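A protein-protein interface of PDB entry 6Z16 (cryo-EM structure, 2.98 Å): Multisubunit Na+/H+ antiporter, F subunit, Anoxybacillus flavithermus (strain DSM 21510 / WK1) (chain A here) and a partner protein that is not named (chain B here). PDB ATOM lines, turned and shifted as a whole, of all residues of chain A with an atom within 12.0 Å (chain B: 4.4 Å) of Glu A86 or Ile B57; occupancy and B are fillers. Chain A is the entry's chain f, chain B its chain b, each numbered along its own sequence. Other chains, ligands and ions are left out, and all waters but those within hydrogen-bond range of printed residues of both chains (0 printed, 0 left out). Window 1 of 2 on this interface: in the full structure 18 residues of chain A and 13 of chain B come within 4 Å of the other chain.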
ATOM      1  N   VAL A  73      -3.890  23.030   3.167  1.00  0.00           N
ATOM      2  CA  VAL A  73      -3.936  23.540   1.797  1.00  0.00           C
ATOM      3  C   VAL A  73      -4.874  24.737   1.700  1.00  0.00           C
ATOM      4  O   VAL A  73      -4.636  25.646   0.893  1.00  0.00           O
ATOM      5  CB  VAL A  73      -4.301  22.440   0.777  1.00  0.00           C
ATOM      6  CG1 VAL A  73      -3.314  21.317   0.852  1.00  0.00           C
ATOM      7  CG2 VAL A  73      -5.704  21.913   0.961  1.00  0.00           C
ATOM      8  N   ALA A  74      -5.891  24.810   2.572  1.00  0.00           N
ATOM      9  CA  ALA A  74      -6.772  25.973   2.594  1.00  0.00           C
ATOM     10  C   ALA A  74      -6.032  27.226   3.046  1.00  0.00           C
ATOM     11  O   ALA A  74      -6.110  28.274   2.390  1.00  0.00           O
ATOM     12  CB  ALA A  74      -7.969  25.703   3.497  1.00  0.00           C
ATOM     13  N   ALA A  76      -2.746  27.688   3.124  1.00  0.00           N
ATOM     14  CA  ALA A  76      -1.688  27.967   2.162  1.00  0.00           C
ATOM     15  C   ALA A  76      -2.228  28.640   0.914  1.00  0.00           C
ATOM     16  O   ALA A  76      -1.525  29.442   0.293  1.00  0.00           O
ATOM     17  CB  ALA A  76      -0.973  26.677   1.779  1.00  0.00           C
ATOM     18  N   LYS A  77      -3.462  28.319   0.521  1.00  0.00           N
ATOM     19  CA  LYS A  77      -4.092  29.075  -0.551  1.00  0.00           C
ATOM     20  C   LYS A  77      -4.460  30.479  -0.087  1.00  0.00           C
ATOM     21  O   LYS A  77      -4.415  31.422  -0.886  1.00  0.00           O
ATOM     22  CB  LYS A  77      -5.317  28.316  -1.066  1.00  0.00           C
ATOM     23  CG  LYS A  77      -6.013  28.956  -2.255  1.00  0.00           C
ATOM     24  CD  LYS A  77      -5.129  28.973  -3.488  1.00  0.00           C
ATOM     25  CE  LYS A  77      -5.815  29.681  -4.644  1.00  0.00           C
ATOM     26  NZ  LYS A  77      -7.023  28.953  -5.115  1.00  0.00           N
ATOM     27  N   PHE A  78      -4.781  30.640   1.203  1.00  0.00           N
ATOM     28  CA  PHE A  78      -5.135  31.964   1.715  1.00  0.00           C
ATOM     29  C   PHE A  78      -3.946  32.917   1.731  1.00  0.00           C
ATOM     30  O   PHE A  78      -4.098  34.098   1.398  1.00  0.00           O
ATOM     31  CB  PHE A  78      -5.729  31.881   3.116  1.00  0.00           C
ATOM     32  CG  PHE A  78      -5.984  33.228   3.716  1.00  0.00           C
ATOM     33  CD1 PHE A  78      -6.920  34.077   3.150  1.00  0.00           C
ATOM     34  CD2 PHE A  78      -5.285  33.652   4.831  1.00  0.00           C
ATOM     35  CE1 PHE A  78      -7.147  35.329   3.675  1.00  0.00           C
ATOM     36  CE2 PHE A  78      -5.515  34.903   5.371  1.00  0.00           C
ATOM     37  CZ  PHE A  78      -6.449  35.742   4.791  1.00  0.00           C
ATOM     38  N   LEU A  79      -2.763  32.437   2.123  1.00  0.00           N
ATOM     39  CA  LEU A  79      -1.594  33.317   2.157  1.00  0.00           C
ATOM     40  C   LEU A  79      -1.128  33.738   0.772  1.00  0.00           C
ATOM     41  O   LEU A  79      -0.377  34.710   0.655  1.00  0.00           O
ATOM     42  CB  LEU A  79      -0.426  32.650   2.869  1.00  0.00           C
ATOM     43  CG  LEU A  79      -0.546  32.377   4.357  1.00  0.00           C
ATOM     44  CD1 LEU A  79       0.714  31.693   4.802  1.00  0.00           C
ATOM     45  CD2 LEU A  79      -0.753  33.666   5.115  1.00  0.00           C
ATOM     46  N   GLU A  80      -1.544  33.030  -0.267  1.00  0.00           N
ATOM     47  CA  GLU A  80      -1.133  33.319  -1.632  1.00  0.00           C
ATOM     48  C   GLU A  80      -2.265  34.042  -2.350  1.00  0.00           C
ATOM     49  O   GLU A  80      -3.248  33.420  -2.765  1.00  0.00           O
ATOM     50  CB  GLU A  80      -0.735  32.034  -2.351  1.00  0.00           C
ATOM     51  CG  GLU A  80      -0.262  32.235  -3.784  1.00  0.00           C
ATOM     52  CD  GLU A  80       1.028  33.026  -3.880  1.00  0.00           C
ATOM     53  OE1 GLU A  80       1.819  33.004  -2.915  1.00  0.00           O
ATOM     54  OE2 GLU A  80       1.255  33.670  -4.927  1.00  0.00           O
ATOM     55  N   LYS A  81      -2.125  35.368  -2.448  1.00  0.00           N
ATOM     56  CA  LYS A  81      -2.891  36.226  -3.360  1.00  0.00           C
ATOM     57  C   LYS A  81      -4.388  36.224  -3.050  1.00  0.00           C
ATOM     58  O   LYS A  81      -5.231  36.141  -3.946  1.00  0.00           O
ATOM     59  CB  LYS A  81      -2.621  35.846  -4.819  1.00  0.00           C
ATOM     60  CG  LYS A  81      -1.197  36.155  -5.260  1.00  0.00           C
ATOM     61  CD  LYS A  81      -0.939  35.799  -6.717  1.00  0.00           C
ATOM     62  CE  LYS A  81       0.504  36.118  -7.106  1.00  0.00           C
ATOM     63  NZ  LYS A  81       0.824  35.766  -8.517  1.00  0.00           N
ATOM     64  N   GLY A  82      -4.717  36.320  -1.765  1.00  0.00           N
ATOM     65  CA  GLY A  82      -6.084  36.607  -1.382  1.00  0.00           C
ATOM     66  C   GLY A  82      -6.982  35.425  -1.087  1.00  0.00           C
ATOM     67  O   GLY A  82      -7.007  34.915   0.036  1.00  0.00           O
ATOM     68  N   VAL A  83      -7.745  35.001  -2.099  1.00  0.00           N
ATOM     69  CA  VAL A  83      -8.879  34.102  -1.901  1.00  0.00           C
ATOM     70  C   VAL A  83      -8.415  32.685  -1.579  1.00  0.00           C
ATOM     71  O   VAL A  83      -7.292  32.272  -1.888  1.00  0.00           O
ATOM     72  CB  VAL A  83      -9.773  34.115  -3.151  1.00  0.00           C
ATOM     73  CG1 VAL A  83     -10.312  35.502  -3.398  1.00  0.00           C
ATOM     74  CG2 VAL A  83      -8.988  33.646  -4.364  1.00  0.00           C
ATOM     75  N   VAL A  84      -9.306  31.929  -0.937  1.00  0.00           N
ATOM     76  CA  VAL A  84      -9.151  30.482  -0.845  1.00  0.00           C
ATOM     77  C   VAL A  84      -9.927  29.763  -1.943  1.00  0.00           C
ATOM     78  O   VAL A  84      -9.604  28.607  -2.257  1.00  0.00           O
ATOM     79  CB  VAL A  84      -9.585  29.938   0.533  1.00  0.00           C
ATOM     80  CG1 VAL A  84      -8.776  30.555   1.621  1.00  0.00           C
ATOM     81  CG2 VAL A  84     -11.056  30.183   0.785  1.00  0.00           C
ATOM     82  N   ILE A  85     -10.946  30.400  -2.519  1.00  0.00           N
ATOM     83  CA  ILE A  85     -11.799  29.817  -3.547  1.00  0.00           C
ATOM     84  C   ILE A  85     -12.001  30.883  -4.612  1.00  0.00           C
ATOM     85  O   ILE A  85     -12.594  31.931  -4.335  1.00  0.00           O
ATOM     86  CB  ILE A  85     -13.156  29.347  -2.990  1.00  0.00           C
ATOM     87  CG1 ILE A  85     -12.978  28.176  -2.021  1.00  0.00           C
ATOM     88  CG2 ILE A  85     -14.084  28.961  -4.119  1.00  0.00           C
ATOM     89  CD1 ILE A  85     -14.201  27.856  -1.215  1.00  0.00           C
ATOM     90  N   GLU A  86     -11.501  30.632  -5.815  1.00  0.00           N
ATOM     91  CA  GLU A  86     -11.522  31.645  -6.855  1.00  0.00           C
ATOM     92  C   GLU A  86     -12.929  31.810  -7.421  1.00  0.00           C
ATOM     93  O   GLU A  86     -13.834  31.015  -7.165  1.00  0.00           O
ATOM     94  CB  GLU A  86     -10.550  31.288  -7.977  1.00  0.00           C
ATOM     95  CG  GLU A  86      -9.094  31.298  -7.565  1.00  0.00           C
ATOM     96  CD  GLU A  86      -8.171  30.906  -8.698  1.00  0.00           C
ATOM     97  OE1 GLU A  86      -8.679  30.544  -9.779  1.00  0.00           O
ATOM     98  OE2 GLU A  86      -6.939  30.948  -8.503  1.00  0.00           O
ATOM     99  N   ARG A  87     -13.102  32.872  -8.198  1.00  0.00           N
ATOM    100  CA  ARG A  87     -14.341  33.136  -8.909  1.00  0.00           C
ATOM    101  C   ARG A  87     -14.220  32.681 -10.357  1.00  0.00           C
ATOM    102  O   ARG A  87     -13.126  32.599 -10.920  1.00  0.00           O
ATOM    103  CB  ARG A  87     -14.695  34.624  -8.854  1.00  0.00           C
ATOM    104  CG  ARG A  87     -15.050  35.127  -7.467  1.00  0.00           C
ATOM    105  CD  ARG A  87     -15.381  36.604  -7.492  1.00  0.00           C
ATOM    106  NE  ARG A  87     -16.556  36.877  -8.313  1.00  0.00           N
ATOM    107  CZ  ARG A  87     -17.806  36.839  -7.865  1.00  0.00           C
ATOM    108  NH1 ARG A  87     -18.048  36.540  -6.599  1.00  0.00           N
ATOM    109  NH2 ARG A  87     -18.815  37.100  -8.683  1.00  0.00           N
ATOM    110  N   GLY A  88     -15.369  32.385 -10.955  1.00  0.00           N
ATOM    111  CA  GLY A  88     -15.384  31.889 -12.315  1.00  0.00           C
ATOM    112  C   GLY A  88     -15.024  32.957 -13.328  1.00  0.00           C
ATOM    113  O   GLY A  88     -15.310  34.142 -13.155  1.00  0.00           O
ATOM    114  N   ASN A  89     -14.377  32.522 -14.401  1.00  0.00           N
ATOM    115  CA  ASN A  89     -13.945  33.424 -15.456  1.00  0.00           C
ATOM    116  C   ASN A  89     -15.116  33.951 -16.288  1.00  0.00           C
ATOM    117  O   ASN A  89     -16.210  33.388 -16.259  1.00  0.00           O
ATOM    118  CB  ASN A  89     -12.911  32.728 -16.350  1.00  0.00           C
ATOM    119  CG  ASN A  89     -13.409  31.405 -16.922  1.00  0.00           C
ATOM    120  OD1 ASN A  89     -14.556  31.006 -16.728  1.00  0.00           O
ATOM    121  ND2 ASN A  89     -12.530  30.715 -17.635  1.00  0.00           N
ATOM    122  N   LEU B  52     -12.627  22.025  -4.672  1.00  0.00           N
ATOM    123  CA  LEU B  52     -12.805  23.476  -4.737  1.00  0.00           C
ATOM    124  C   LEU B  52     -11.508  24.219  -4.469  1.00  0.00           C
ATOM    125  O   LEU B  52     -11.285  25.298  -5.025  1.00  0.00           O
ATOM    126  CB  LEU B  52     -13.853  23.935  -3.725  1.00  0.00           C
ATOM    127  CG  LEU B  52     -15.321  23.636  -3.975  1.00  0.00           C
ATOM    128  CD1 LEU B  52     -16.118  23.963  -2.741  1.00  0.00           C
ATOM    129  CD2 LEU B  52     -15.790  24.472  -5.132  1.00  0.00           C
ATOM    130  N   ASP B  56     -11.477  26.045  -9.605  1.00  0.00           N
ATOM    131  CA  ASP B  56     -12.298  27.243  -9.613  1.00  0.00           C
ATOM    132  C   ASP B  56     -13.628  26.933  -8.913  1.00  0.00           C
ATOM    133  O   ASP B  56     -13.774  25.903  -8.253  1.00  0.00           O
ATOM    134  CB  ASP B  56     -12.446  27.715 -11.061  1.00  0.00           C
ATOM    135  CG  ASP B  56     -12.820  29.174 -11.177  1.00  0.00           C
ATOM    136  OD1 ASP B  56     -13.016  29.817 -10.127  1.00  0.00           O
ATOM    137  OD2 ASP B  56     -12.912  29.672 -12.316  1.00  0.00           O
ATOM    138  N   ILE B  57     -14.609  27.829  -9.025  1.00  0.00           N
ATOM    139  CA  ILE B  57     -15.941  27.609  -8.471  1.00  0.00           C
ATOM    140  C   ILE B  57     -16.869  27.145  -9.589  1.00  0.00           C
ATOM    141  O   ILE B  57     -17.820  26.395  -9.351  1.00  0.00           O
ATOM    142  CB  ILE B  57     -16.463  28.874  -7.751  1.00  0.00           C
ATOM    143  CG1 ILE B  57     -17.766  28.600  -6.991  1.00  0.00           C
ATOM    144  CG2 ILE B  57     -16.600  30.072  -8.698  1.00  0.00           C
ATOM    145  CD1 ILE B  57     -17.611  27.665  -5.829  1.00  0.00           C
ATOM    146  N   GLU B  58     -16.582  27.555 -10.828  1.00  0.00           N
ATOM    147  CA  GLU B  58     -17.374  27.090 -11.958  1.00  0.00           C
ATOM    148  C   GLU B  58     -16.872  25.751 -12.476  1.00  0.00           C
ATOM    149  O   GLU B  58     -17.658  24.957 -13.008  1.00  0.00           O
ATOM    150  CB  GLU B  58     -17.375  28.149 -13.068  1.00  0.00           C
ATOM    151  CG  GLU B  58     -16.006  28.512 -13.632  1.00  0.00           C
ATOM    152  CD  GLU B  58     -15.623  27.705 -14.859  1.00  0.00           C
ATOM    153  OE1 GLU B  58     -16.529  27.182 -15.539  1.00  0.00           O
ATOM    154  OE2 GLU B  58     -14.412  27.590 -15.141  1.00  0.00           O
ATOM    155  N   THR B  59     -15.577  25.481 -12.308  1.00  0.00           N
ATOM    156  CA  THR B  59     -15.006  24.233 -12.787  1.00  0.00           C
ATOM    157  C   THR B  59     -15.487  23.057 -11.953  1.00  0.00           C
ATOM    158  O   THR B  59     -15.709  21.974 -12.491  1.00  0.00           O
ATOM    159  CB  THR B  59     -13.478  24.334 -12.776  1.00  0.00           C
ATOM    160  OG1 THR B  59     -13.076  25.489 -13.523  1.00  0.00           O
ATOM    161  CG2 THR B  59     -12.838  23.117 -13.415  1.00  0.00           C
ATOM    162  N   VAL B  60     -15.716  23.262 -10.659  1.00  0.00           N
ATOM    163  CA  VAL B  60     -16.154  22.161  -9.807  1.00  0.00           C
ATOM    164  C   VAL B  60     -17.624  21.835 -10.044  1.00  0.00           C
ATOM    165  O   VAL B  60     -18.009  20.660 -10.087  1.00  0.00           O
ATOM    166  CB  VAL B  60     -15.856  22.497  -8.337  1.00  0.00           C
ATOM    167  CG1 VAL B  60     -16.383  21.421  -7.407  1.00  0.00           C
ATOM    168  CG2 VAL B  60     -14.369  22.648  -8.156  1.00  0.00           C
ATOM    169  N   ARG B  61     -18.468  22.848 -10.250  1.00  0.00           N
ATOM    170  CA  ARG B  61     -19.842  22.551 -10.635  1.00  0.00           C
ATOM    171  C   ARG B  61     -19.941  22.065 -12.073  1.00  0.00           C
ATOM    172  O   ARG B  61     -20.963  21.483 -12.445  1.00  0.00           O
ATOM    173  CB  ARG B  61     -20.758  23.761 -10.438  1.00  0.00           C
ATOM    174  CG  ARG B  61     -20.461  24.950 -11.324  1.00  0.00           C
ATOM    175  CD  ARG B  61     -21.598  25.957 -11.265  1.00  0.00           C
ATOM    176  NE  ARG B  61     -21.820  26.502  -9.931  1.00  0.00           N
ATOM    177  CZ  ARG B  61     -21.279  27.626  -9.483  1.00  0.00           C
ATOM    178  NH1 ARG B  61     -20.487  28.340 -10.270  1.00  0.00           N
ATOM    179  NH2 ARG B  61     -21.542  28.044  -8.253  1.00  0.00           N
ATOM    180  N   GLU B 134     -20.104  27.144  -1.056  1.00  0.00           N
ATOM    181  CA  GLU B 134     -20.093  27.842  -2.336  1.00  0.00           C
ATOM    182  C   GLU B 134     -21.011  29.056  -2.357  1.00  0.00           C
ATOM    183  O   GLU B 134     -20.998  29.788  -3.347  1.00  0.00           O
ATOM    184  CB  GLU B 134     -20.462  26.912  -3.496  1.00  0.00           C
ATOM    185  CG  GLU B 134     -21.936  26.592  -3.646  1.00  0.00           C
ATOM    186  CD  GLU B 134     -22.199  25.603  -4.768  1.00  0.00           C
ATOM    187  OE1 GLU B 134     -21.224  25.190  -5.431  1.00  0.00           O
ATOM    188  OE2 GLU B 134     -23.371  25.227  -4.979  1.00  0.00           O
ATOM    189  N   GLU B 138     -18.621  32.729  -3.548  1.00  0.00           N
ATOM    190  CA  GLU B 138     -18.906  33.602  -4.679  1.00  0.00           C
ATOM    191  C   GLU B 138     -19.666  34.860  -4.272  1.00  0.00           C
ATOM    192  O   GLU B 138     -20.278  35.512  -5.125  1.00  0.00           O
ATOM    193  CB  GLU B 138     -19.676  32.830  -5.751  1.00  0.00           C
ATOM    194  CG  GLU B 138     -21.043  32.339  -5.311  1.00  0.00           C
ATOM    195  CD  GLU B 138     -21.691  31.423  -6.329  1.00  0.00           C
ATOM    196  OE1 GLU B 138     -21.083  31.182  -7.391  1.00  0.00           O
ATOM    197  OE2 GLU B 138     -22.805  30.930  -6.062  1.00  0.00           O
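O of Glu B138 is in hydrogen-bond range of NH1 of Arg A87 (2.9 Å).
O of Glu A86 sits close to OD1 of Asp B56, 3.3 Å away.
The backbone carbonyl oxygen (O) of Arg A87 sits close to the side-chain carboxylate (OD1) of Asp B56.
The backbone carbonyl oxygen (O) of Ile B57 sits at hydrogen-bond distance from the guanidinium group (NH1) of Arg B61 (3.4 Å).
The side-chain hydroxyl (OG1) of Thr B59 lies within hydrogen-bond range of the side-chain carboxylate (OE2) of Glu B58 (3.0 Å).
The side-chain carboxylate (OE1) of Glu B138 is in salt-bridge range of the guanidinium group (NH2) of Arg B61.
The side-chain amino group (NZ) of Lys A77 is in salt-bridge range of the side-chain carboxylate (OE2) of Glu A86 (3.9 Å).
Among the printed residues, merely in contact across the chains: Glu A86 with Ile B57 (3.3 Å), Gly A88 with Asp B56 (3.3 Å), Gly A88 with Ile B57 (3.5 Å), Gly A88 with Glu B58 (3.7 Å), Asn A89 with Glu B58 (3.8 Å), Arg A87 with Ile B57 (3.8 Å) and Asn A89 with Asp B56 (3.8 Å).
Glu A80 touches none of the printed residues of chain B.
Val A83 touches none of the printed residues of chain B.
Glu A86 touches just these residues of chain B: Asp B56 (3.3 Å) and Ile B57 (3.3 Å).
Of the printed residues of chain B, Arg A87 touches Asp B56, Ile B57 and Glu B138.
Printed residues of chain B within 4 Å of Gly A88: Asp B56 (3.3 Å), Ile B57 (3.5 Å) and Glu B58 (3.7 Å).
Leu B52 touches none of the printed residues of chain A.
Asp B56 touches just these residues of chain A: Glu A86 (3.3 Å), Arg A87 (2.9 Å), Gly A88 (3.3 Å) and Asn A89 (3.8 Å).
Glu B58 touches just these residues of chain A: Gly A88 and Asn A89.
No residue of chain A comes within 4 Å of Thr B59.
No residue of chain A comes within 4 Å of Val B60.
No residue of chain A comes within 4 Å of Arg B61.
No residue of chain A comes within 4 Å of Glu B134.
The nearest printed residue of chain B that does not touch Glu A86 is Leu B52 (5.4 Å).
The nearest residue of chain A that does not touch Ile B57 is Ile A85 (4.1 Å).
Of the 9 printed residues of chain B, 4 touch a printed residue of chain A.
Printed residues of chain B that touch a printed residue of chain A: Asp B56, Ile B57, Glu B58 and Glu B138.
Hydrophobic or aromatic side chains of chain B within 4 Å of the printed part of chain A: Ile B57.
Of the 16 printed residues of chain A, 4 touch a printed residue of chain B.
Printed residues of chain A that touch a printed residue of chain B: Glu A86, Arg A87, Gly A88 and Asn A89.
Along chain A the printed residues that touch a printed residue of chain B span positions 86 to 89.
Among the printed residues, 10 pairs touch across the chains.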
